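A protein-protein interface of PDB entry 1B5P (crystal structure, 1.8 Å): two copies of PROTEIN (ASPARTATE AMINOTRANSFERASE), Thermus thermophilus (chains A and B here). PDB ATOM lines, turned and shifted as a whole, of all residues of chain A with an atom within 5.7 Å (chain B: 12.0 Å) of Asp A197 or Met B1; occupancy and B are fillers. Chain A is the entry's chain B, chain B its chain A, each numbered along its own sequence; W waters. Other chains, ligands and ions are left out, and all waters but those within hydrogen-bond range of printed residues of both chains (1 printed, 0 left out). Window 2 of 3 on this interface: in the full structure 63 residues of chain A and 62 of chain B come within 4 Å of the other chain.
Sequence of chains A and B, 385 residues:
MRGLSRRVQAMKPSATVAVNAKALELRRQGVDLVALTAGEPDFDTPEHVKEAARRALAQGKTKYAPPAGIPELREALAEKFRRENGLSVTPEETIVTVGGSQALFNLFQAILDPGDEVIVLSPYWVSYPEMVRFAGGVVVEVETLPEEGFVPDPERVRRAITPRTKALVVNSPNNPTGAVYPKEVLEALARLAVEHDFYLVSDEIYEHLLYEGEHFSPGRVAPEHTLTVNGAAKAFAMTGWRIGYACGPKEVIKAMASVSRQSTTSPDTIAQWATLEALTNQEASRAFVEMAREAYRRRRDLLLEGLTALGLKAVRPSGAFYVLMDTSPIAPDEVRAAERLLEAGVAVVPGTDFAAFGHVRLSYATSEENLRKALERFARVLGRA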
ATOM      1  N   PRO A 163     -19.598  15.417 -15.281  1.00  0.00           N
ATOM      2  CA  PRO A 163     -20.675  14.661 -14.638  1.00  0.00           C
ATOM      3  C   PRO A 163     -20.507  14.474 -13.114  1.00  0.00           C
ATOM      4  O   PRO A 163     -21.469  14.119 -12.427  1.00  0.00           O
ATOM      5  CB  PRO A 163     -20.657  13.340 -15.409  1.00  0.00           C
ATOM      6  CG  PRO A 163     -20.196  13.771 -16.792  1.00  0.00           C
ATOM      7  CD  PRO A 163     -19.060  14.691 -16.443  1.00  0.00           C
ATOM      8  N   ARG A 164     -19.315  14.754 -12.578  1.00  0.00           N
ATOM      9  CA  ARG A 164     -19.069  14.613 -11.143  1.00  0.00           C
ATOM     10  C   ARG A 164     -19.222  15.909 -10.373  1.00  0.00           C
ATOM     11  O   ARG A 164     -19.010  15.934  -9.157  1.00  0.00           O
ATOM     12  CB  ARG A 164     -17.653  14.129 -10.888  1.00  0.00           C
ATOM     13  CG  ARG A 164     -17.225  13.013 -11.769  1.00  0.00           C
ATOM     14  CD  ARG A 164     -17.520  11.685 -11.123  1.00  0.00           C
ATOM     15  NE  ARG A 164     -18.913  11.542 -10.711  1.00  0.00           N
ATOM     16  CZ  ARG A 164     -19.292  11.127  -9.500  1.00  0.00           C
ATOM     17  NH1 ARG A 164     -18.380  10.819  -8.566  1.00  0.00           N
ATOM     18  NH2 ARG A 164     -20.588  10.995  -9.225  1.00  0.00           N
ATOM     19  N   THR A 165     -19.511  17.006 -11.070  1.00  0.00           N
ATOM     20  CA  THR A 165     -19.646  18.279 -10.372  1.00  0.00           C
ATOM     21  C   THR A 165     -20.831  18.271  -9.417  1.00  0.00           C
ATOM     22  O   THR A 165     -21.979  18.120  -9.837  1.00  0.00           O
ATOM     23  CB  THR A 165     -19.821  19.467 -11.311  1.00  0.00           C
ATOM     24  OG1 THR A 165     -18.834  19.426 -12.344  1.00  0.00           O
ATOM     25  CG2 THR A 165     -19.668  20.764 -10.518  1.00  0.00           C
ATOM     26  N   LYS A 166     -20.523  18.491  -8.146  1.00  0.00           N
ATOM     27  CA  LYS A 166     -21.488  18.539  -7.047  1.00  0.00           C
ATOM     28  C   LYS A 166     -21.835  19.971  -6.659  1.00  0.00           C
ATOM     29  O   LYS A 166     -22.961  20.258  -6.259  1.00  0.00           O
ATOM     30  CB  LYS A 166     -20.858  17.919  -5.802  1.00  0.00           C
ATOM     31  CG  LYS A 166     -21.641  16.826  -5.129  1.00  0.00           C
ATOM     32  CD  LYS A 166     -23.113  17.112  -5.022  1.00  0.00           C
ATOM     33  CE  LYS A 166     -23.839  15.789  -5.047  1.00  0.00           C
ATOM     34  NZ  LYS A 166     -23.286  14.899  -4.002  1.00  0.00           N
ATOM     35  N   ALA A 167     -20.820  20.828  -6.691  1.00  0.00           N
ATOM     36  CA  ALA A 167     -20.950  22.220  -6.285  1.00  0.00           C
ATOM     37  C   ALA A 167     -20.012  23.212  -6.970  1.00  0.00           C
ATOM     38  O   ALA A 167     -18.954  22.841  -7.478  1.00  0.00           O
ATOM     39  CB  ALA A 167     -20.726  22.317  -4.780  1.00  0.00           C
ATOM     40  N   LEU A 192     -26.320  27.806 -14.681  1.00  0.00           N
ATOM     41  CA  LEU A 192     -25.482  26.633 -14.937  1.00  0.00           C
ATOM     42  C   LEU A 192     -25.816  25.530 -13.925  1.00  0.00           C
ATOM     43  O   LEU A 192     -25.902  24.358 -14.292  1.00  0.00           O
ATOM     44  CB  LEU A 192     -23.995  26.983 -14.853  1.00  0.00           C
ATOM     45  CG  LEU A 192     -23.404  27.847 -15.968  1.00  0.00           C
ATOM     46  CD1 LEU A 192     -21.985  28.245 -15.597  1.00  0.00           C
ATOM     47  CD2 LEU A 192     -23.433  27.096 -17.294  1.00  0.00           C
ATOM     48  N   ALA A 193     -26.000  25.920 -12.660  1.00  0.00           N
ATOM     49  CA  ALA A 193     -26.340  24.995 -11.582  1.00  0.00           C
ATOM     50  C   ALA A 193     -27.655  24.277 -11.852  1.00  0.00           C
ATOM     51  O   ALA A 193     -27.794  23.086 -11.587  1.00  0.00           O
ATOM     52  CB  ALA A 193     -26.423  25.746 -10.263  1.00  0.00           C
ATOM     53  N   VAL A 194     -28.631  25.030 -12.348  1.00  0.00           N
ATOM     54  CA  VAL A 194     -29.943  24.489 -12.667  1.00  0.00           C
ATOM     55  C   VAL A 194     -29.855  23.572 -13.880  1.00  0.00           C
ATOM     56  O   VAL A 194     -30.384  22.462 -13.874  1.00  0.00           O
ATOM     57  CB  VAL A 194     -30.946  25.627 -12.969  1.00  0.00           C
ATOM     58  CG1 VAL A 194     -32.220  25.062 -13.586  1.00  0.00           C
ATOM     59  CG2 VAL A 194     -31.260  26.392 -11.696  1.00  0.00           C
ATOM     60  N   GLU A 195     -29.167  24.036 -14.914  1.00  0.00           N
ATOM     61  CA  GLU A 195     -29.018  23.263 -16.139  1.00  0.00           C
ATOM     62  C   GLU A 195     -28.211  22.003 -15.949  1.00  0.00           C
ATOM     63  O   GLU A 195     -28.491  20.985 -16.588  1.00  0.00           O
ATOM     64  CB  GLU A 195     -28.339  24.090 -17.210  1.00  0.00           C
ATOM     65  CG  GLU A 195     -29.302  24.936 -17.981  1.00  0.00           C
ATOM     66  CD  GLU A 195     -28.627  26.119 -18.612  1.00  0.00           C
ATOM     67  OE1 GLU A 195     -27.378  26.213 -18.568  1.00  0.00           O
ATOM     68  OE2 GLU A 195     -29.347  26.978 -19.149  1.00  0.00           O
ATOM     69  N   HIS A 196     -27.189  22.078 -15.104  1.00  0.00           N
ATOM     70  CA  HIS A 196     -26.345  20.917 -14.884  1.00  0.00           C
ATOM     71  C   HIS A 196     -26.603  20.202 -13.574  1.00  0.00           C
ATOM     72  O   HIS A 196     -25.879  19.268 -13.225  1.00  0.00           O
ATOM     73  CB  HIS A 196     -24.879  21.285 -15.056  1.00  0.00           C
ATOM     74  CG  HIS A 196     -24.559  21.793 -16.425  1.00  0.00           C
ATOM     75  ND1 HIS A 196     -24.516  23.137 -16.723  1.00  0.00           N
ATOM     76  CD2 HIS A 196     -24.326  21.138 -17.589  1.00  0.00           C
ATOM     77  CE1 HIS A 196     -24.273  23.293 -18.015  1.00  0.00           C
ATOM     78  NE2 HIS A 196     -24.155  22.099 -18.562  1.00  0.00           N
ATOM     79  N   ASP A 197     -27.613  20.651 -12.837  1.00  0.00           N
ATOM     80  CA  ASP A 197     -27.985  19.978 -11.609  1.00  0.00           C
ATOM     81  C   ASP A 197     -26.928  19.866 -10.514  1.00  0.00           C
ATOM     82  O   ASP A 197     -26.564  18.764 -10.134  1.00  0.00           O
ATOM     83  CB  ASP A 197     -28.456  18.575 -11.989  1.00  0.00           C
ATOM     84  CG  ASP A 197     -29.356  17.947 -10.954  1.00  0.00           C
ATOM     85  OD1 ASP A 197     -29.383  18.397  -9.787  1.00  0.00           O
ATOM     86  OD2 ASP A 197     -30.041  16.976 -11.324  1.00  0.00           O
ATOM     87  N   PHE A 198     -26.398  20.980 -10.042  1.00  0.00           N
ATOM     88  CA  PHE A 198     -25.443  20.912  -8.948  1.00  0.00           C
ATOM     89  C   PHE A 198     -25.789  22.041  -7.987  1.00  0.00           C
ATOM     90  O   PHE A 198     -26.715  22.808  -8.254  1.00  0.00           O
ATOM     91  CB  PHE A 198     -23.970  20.913  -9.415  1.00  0.00           C
ATOM     92  CG  PHE A 198     -23.576  22.081 -10.278  1.00  0.00           C
ATOM     93  CD1 PHE A 198     -23.345  23.331  -9.715  1.00  0.00           C
ATOM     94  CD2 PHE A 198     -23.361  21.914 -11.643  1.00  0.00           C
ATOM     95  CE1 PHE A 198     -22.901  24.401 -10.496  1.00  0.00           C
ATOM     96  CE2 PHE A 198     -22.917  22.978 -12.428  1.00  0.00           C
ATOM     97  CZ  PHE A 198     -22.686  24.219 -11.853  1.00  0.00           C
ATOM     98  N   TYR A 199     -25.149  22.071  -6.823  1.00  0.00           N
ATOM     99  CA  TYR A 199     -25.429  23.114  -5.841  1.00  0.00           C
ATOM    100  C   TYR A 199     -24.574  24.355  -6.065  1.00  0.00           C
ATOM    101  O   TYR A 199     -23.428  24.266  -6.484  1.00  0.00           O
ATOM    102  CB  TYR A 199     -25.153  22.613  -4.415  1.00  0.00           C
ATOM    103  CG  TYR A 199     -26.035  21.492  -3.933  1.00  0.00           C
ATOM    104  CD1 TYR A 199     -27.384  21.705  -3.642  1.00  0.00           C
ATOM    105  CD2 TYR A 199     -25.513  20.221  -3.740  1.00  0.00           C
ATOM    106  CE1 TYR A 199     -28.186  20.671  -3.161  1.00  0.00           C
ATOM    107  CE2 TYR A 199     -26.304  19.185  -3.263  1.00  0.00           C
ATOM    108  CZ  TYR A 199     -27.635  19.413  -2.978  1.00  0.00           C
ATOM    109  OH  TYR A 199     -28.394  18.371  -2.504  1.00  0.00           O
ATOM    110  N   HIS A 225     -31.323  25.122  -5.538  1.00  0.00           N
ATOM    111  CA  HIS A 225     -29.945  24.764  -5.898  1.00  0.00           C
ATOM    112  C   HIS A 225     -28.932  25.588  -5.137  1.00  0.00           C
ATOM    113  O   HIS A 225     -27.744  25.328  -5.221  1.00  0.00           O
ATOM    114  CB  HIS A 225     -29.647  25.036  -7.373  1.00  0.00           C
ATOM    115  CG  HIS A 225     -30.384  24.148  -8.316  1.00  0.00           C
ATOM    116  ND1 HIS A 225     -31.737  24.242  -8.514  1.00  0.00           N
ATOM    117  CD2 HIS A 225     -29.953  23.134  -9.103  1.00  0.00           C
ATOM    118  CE1 HIS A 225     -32.122  23.326  -9.376  1.00  0.00           C
ATOM    119  NE2 HIS A 225     -31.059  22.637  -9.750  1.00  0.00           N
ATOM    120  N   MET B   1     -24.336  16.628 -10.142  1.00  0.00           N
ATOM    121  CA  MET B   1     -25.618  16.173  -9.528  1.00  0.00           C
ATOM    122  C   MET B   1     -25.796  16.674  -8.084  1.00  0.00           C
ATOM    123  O   MET B   1     -24.836  17.105  -7.454  1.00  0.00           O
ATOM    124  CB  MET B   1     -25.725  14.648  -9.594  1.00  0.00           C
ATOM    125  CG  MET B   1     -27.143  14.121  -9.390  1.00  0.00           C
ATOM    126  SD  MET B   1     -28.412  15.267 -10.005  1.00  0.00           S
ATOM    127  CE  MET B   1     -29.760  15.248  -8.652  1.00  0.00           C
ATOM    128  N   ARG B   2     -27.039  16.686  -7.601  1.00  0.00           N
ATOM    129  CA  ARG B   2     -27.360  17.130  -6.239  1.00  0.00           C
ATOM    130  C   ARG B   2     -27.705  15.964  -5.335  1.00  0.00           C
ATOM    131  O   ARG B   2     -28.092  14.901  -5.808  1.00  0.00           O
ATOM    132  CB  ARG B   2     -28.535  18.105  -6.251  1.00  0.00           C
ATOM    133  CG  ARG B   2     -28.153  19.519  -6.585  1.00  0.00           C
ATOM    134  CD  ARG B   2     -29.373  20.405  -6.560  1.00  0.00           C
ATOM    135  NE  ARG B   2     -30.268  20.005  -7.622  1.00  0.00           N
ATOM    136  CZ  ARG B   2     -31.561  20.289  -7.678  1.00  0.00           C
ATOM    137  NH1 ARG B   2     -32.143  20.999  -6.713  1.00  0.00           N
ATOM    138  NH2 ARG B   2     -32.273  19.849  -8.709  1.00  0.00           N
ATOM    139  N   GLY B   3     -27.590  16.162  -4.032  1.00  0.00           N
ATOM    140  CA  GLY B   3     -27.925  15.072  -3.146  1.00  0.00           C
ATOM    141  C   GLY B   3     -26.989  15.006  -1.975  1.00  0.00           C
ATOM    142  O   GLY B   3     -25.871  15.541  -2.008  1.00  0.00           O
ATOM    143  N   LEU B   4     -27.436  14.294  -0.949  1.00  0.00           N
ATOM    144  CA  LEU B   4     -26.672  14.159   0.270  1.00  0.00           C
ATOM    145  C   LEU B   4     -25.601  13.064   0.218  1.00  0.00           C
ATOM    146  O   LEU B   4     -25.663  12.145  -0.598  1.00  0.00           O
ATOM    147  CB  LEU B   4     -27.642  13.982   1.444  1.00  0.00           C
ATOM    148  CG  LEU B   4     -28.704  15.095   1.608  1.00  0.00           C
ATOM    149  CD1 LEU B   4     -29.668  14.709   2.703  1.00  0.00           C
ATOM    150  CD2 LEU B   4     -28.076  16.461   1.899  1.00  0.00           C
ATOM    151  N   SER B   5     -24.575  13.255   1.036  1.00  0.00           N
ATOM    152  CA  SER B   5     -23.451  12.343   1.142  1.00  0.00           C
ATOM    153  C   SER B   5     -23.876  11.107   1.920  1.00  0.00           C
ATOM    154  O   SER B   5     -24.828  11.153   2.696  1.00  0.00           O
ATOM    155  CB  SER B   5     -22.301  13.015   1.894  1.00  0.00           C
ATOM    156  OG  SER B   5     -22.662  13.239   3.256  1.00  0.00           O
ATOM    157  N   ARG B   6     -23.159  10.000   1.721  1.00  0.00           N
ATOM    158  CA  ARG B   6     -23.453   8.748   2.414  1.00  0.00           C
ATOM    159  C   ARG B   6     -23.238   8.872   3.910  1.00  0.00           C
ATOM    160  O   ARG B   6     -24.002   8.319   4.689  1.00  0.00           O
ATOM    161  CB  ARG B   6     -22.560   7.611   1.909  1.00  0.00           C
ATOM    162  CG  ARG B   6     -22.719   7.282   0.450  1.00  0.00           C
ATOM    163  CD  ARG B   6     -21.847   6.109   0.029  1.00  0.00           C
ATOM    164  NE  ARG B   6     -22.235   5.677  -1.307  1.00  0.00           N
ATOM    165  CZ  ARG B   6     -21.625   6.056  -2.428  1.00  0.00           C
ATOM    166  NH1 ARG B   6     -20.567   6.867  -2.377  1.00  0.00           N
ATOM    167  NH2 ARG B   6     -22.133   5.695  -3.607  1.00  0.00           N
ATOM    168  N   GLN B   9     -26.320  10.358   5.305  1.00  0.00           N
ATOM    169  CA  GLN B   9     -27.509   9.527   5.151  1.00  0.00           C
ATOM    170  C   GLN B   9     -27.404   8.306   6.068  1.00  0.00           C
ATOM    171  O   GLN B   9     -28.417   7.763   6.512  1.00  0.00           O
ATOM    172  CB  GLN B   9     -27.678   9.074   3.694  1.00  0.00           C
ATOM    173  CG  GLN B   9     -28.139  10.181   2.753  1.00  0.00           C
ATOM    174  CD  GLN B   9     -28.500   9.671   1.369  1.00  0.00           C
ATOM    175  OE1 GLN B   9     -27.626   9.450   0.530  1.00  0.00           O
ATOM    176  NE2 GLN B   9     -29.796   9.513   1.112  1.00  0.00           N
HETATM  177  O   HOH W   1     -31.352  20.939 -11.722  1.00  0.00           O
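Of the 14 printed residues of chain A, 6 touch a printed residue of chain B.
Printed residues of chain A that touch a printed residue of chain B: Thr A165, Lys A166, Asp A197, Phe A198, Tyr A199 and His A225.
Hydrophobic or aromatic side chains of chain A that line the printed part of chain B: Tyr A199 and His A225.
Of the 7 printed residues of chain B, 3 touch a printed residue of chain A.
Among the printed residues, 10 pairs touch across the chains.
Among the printed residues, Asp or Glu carboxylates within 4 Å of a Lys or Arg side-chain nitrogen of the other chain: Asp A197 with Arg B2 (2.8 Å).
O of Thr A165 lies within hydrogen-bond range of N of Met B1 (2.8 Å).
N of Met B1 sits close to O of Asp A197, at 3.1 Å.
The guanidinium group (NE) of Arg B2 is in salt-bridge range of the side-chain carboxylate (OD1) of Asp A197 (2.8 Å).
The guanidinium group (NH2) of Arg B2 sits close to a ring nitrogen (NE2) of His A225.
The backbone carbonyl oxygen (O) of Gly B3 lies within hydrogen-bond range of the side-chain amino group (NZ) of Lys A166.
N of Gly B3 is in hydrogen-bond range of OH of Tyr A199, 2.8 Å away.
N of Tyr A199 lies within hydrogen-bond range of O of Lys A166.
The backbone NH of Phe A198 lies within hydrogen-bond range of the backbone carbonyl oxygen of Ala A193, at 3.0 Å.
CE of Lys A166 touches O of Met B1 (2.9 Å).
C of Arg B2 touches CE of Lys A166, 3.9 Å away.
Phe A198 touches Arg B2.
Arg B2 touches Tyr A199 (CD to CE1, 3.6 Å).
Of chain B, only Met B1 comes within 4 Å of Thr A165.
Of chain B, only Met B1 (2.9 Å), Arg B2 (3.9 Å) and Gly B3 (3.3 Å) come within 4 Å of Lys A166.
No residue of chain B comes within 4 Å of Val A194.
His A196 touches none of the printed residues of chain B.
Tyr A199 touches two residues of chain B.
Of the printed residues of chain B, His A225 touches Arg B2 (3.2 Å).
Met B1 touches just these residues of chain A: Thr A165, Lys A166 and Asp A197.
Of the printed residues of chain A, Arg B2 touches Lys A166 (3.9 Å), Asp A197 (2.8 Å), Phe A198 (3.7 Å), Tyr A199 (3.6 Å) and His A225 (3.2 Å).
Of the printed residues of chain A, Gly B3 touches Lys A166 (3.3 Å) and Tyr A199 (2.8 Å).
Gln B9 touches none of the printed residues of chain A.
No position is printed for both chains.
Water W1 lies within hydrogen-bond range of a ring nitrogen (NE2) of His A225 (2.6 Å), the backbone carbonyl oxygen of Val A194 (2.8 Å) and the guanidinium group of Arg B2 (3.3 Å).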
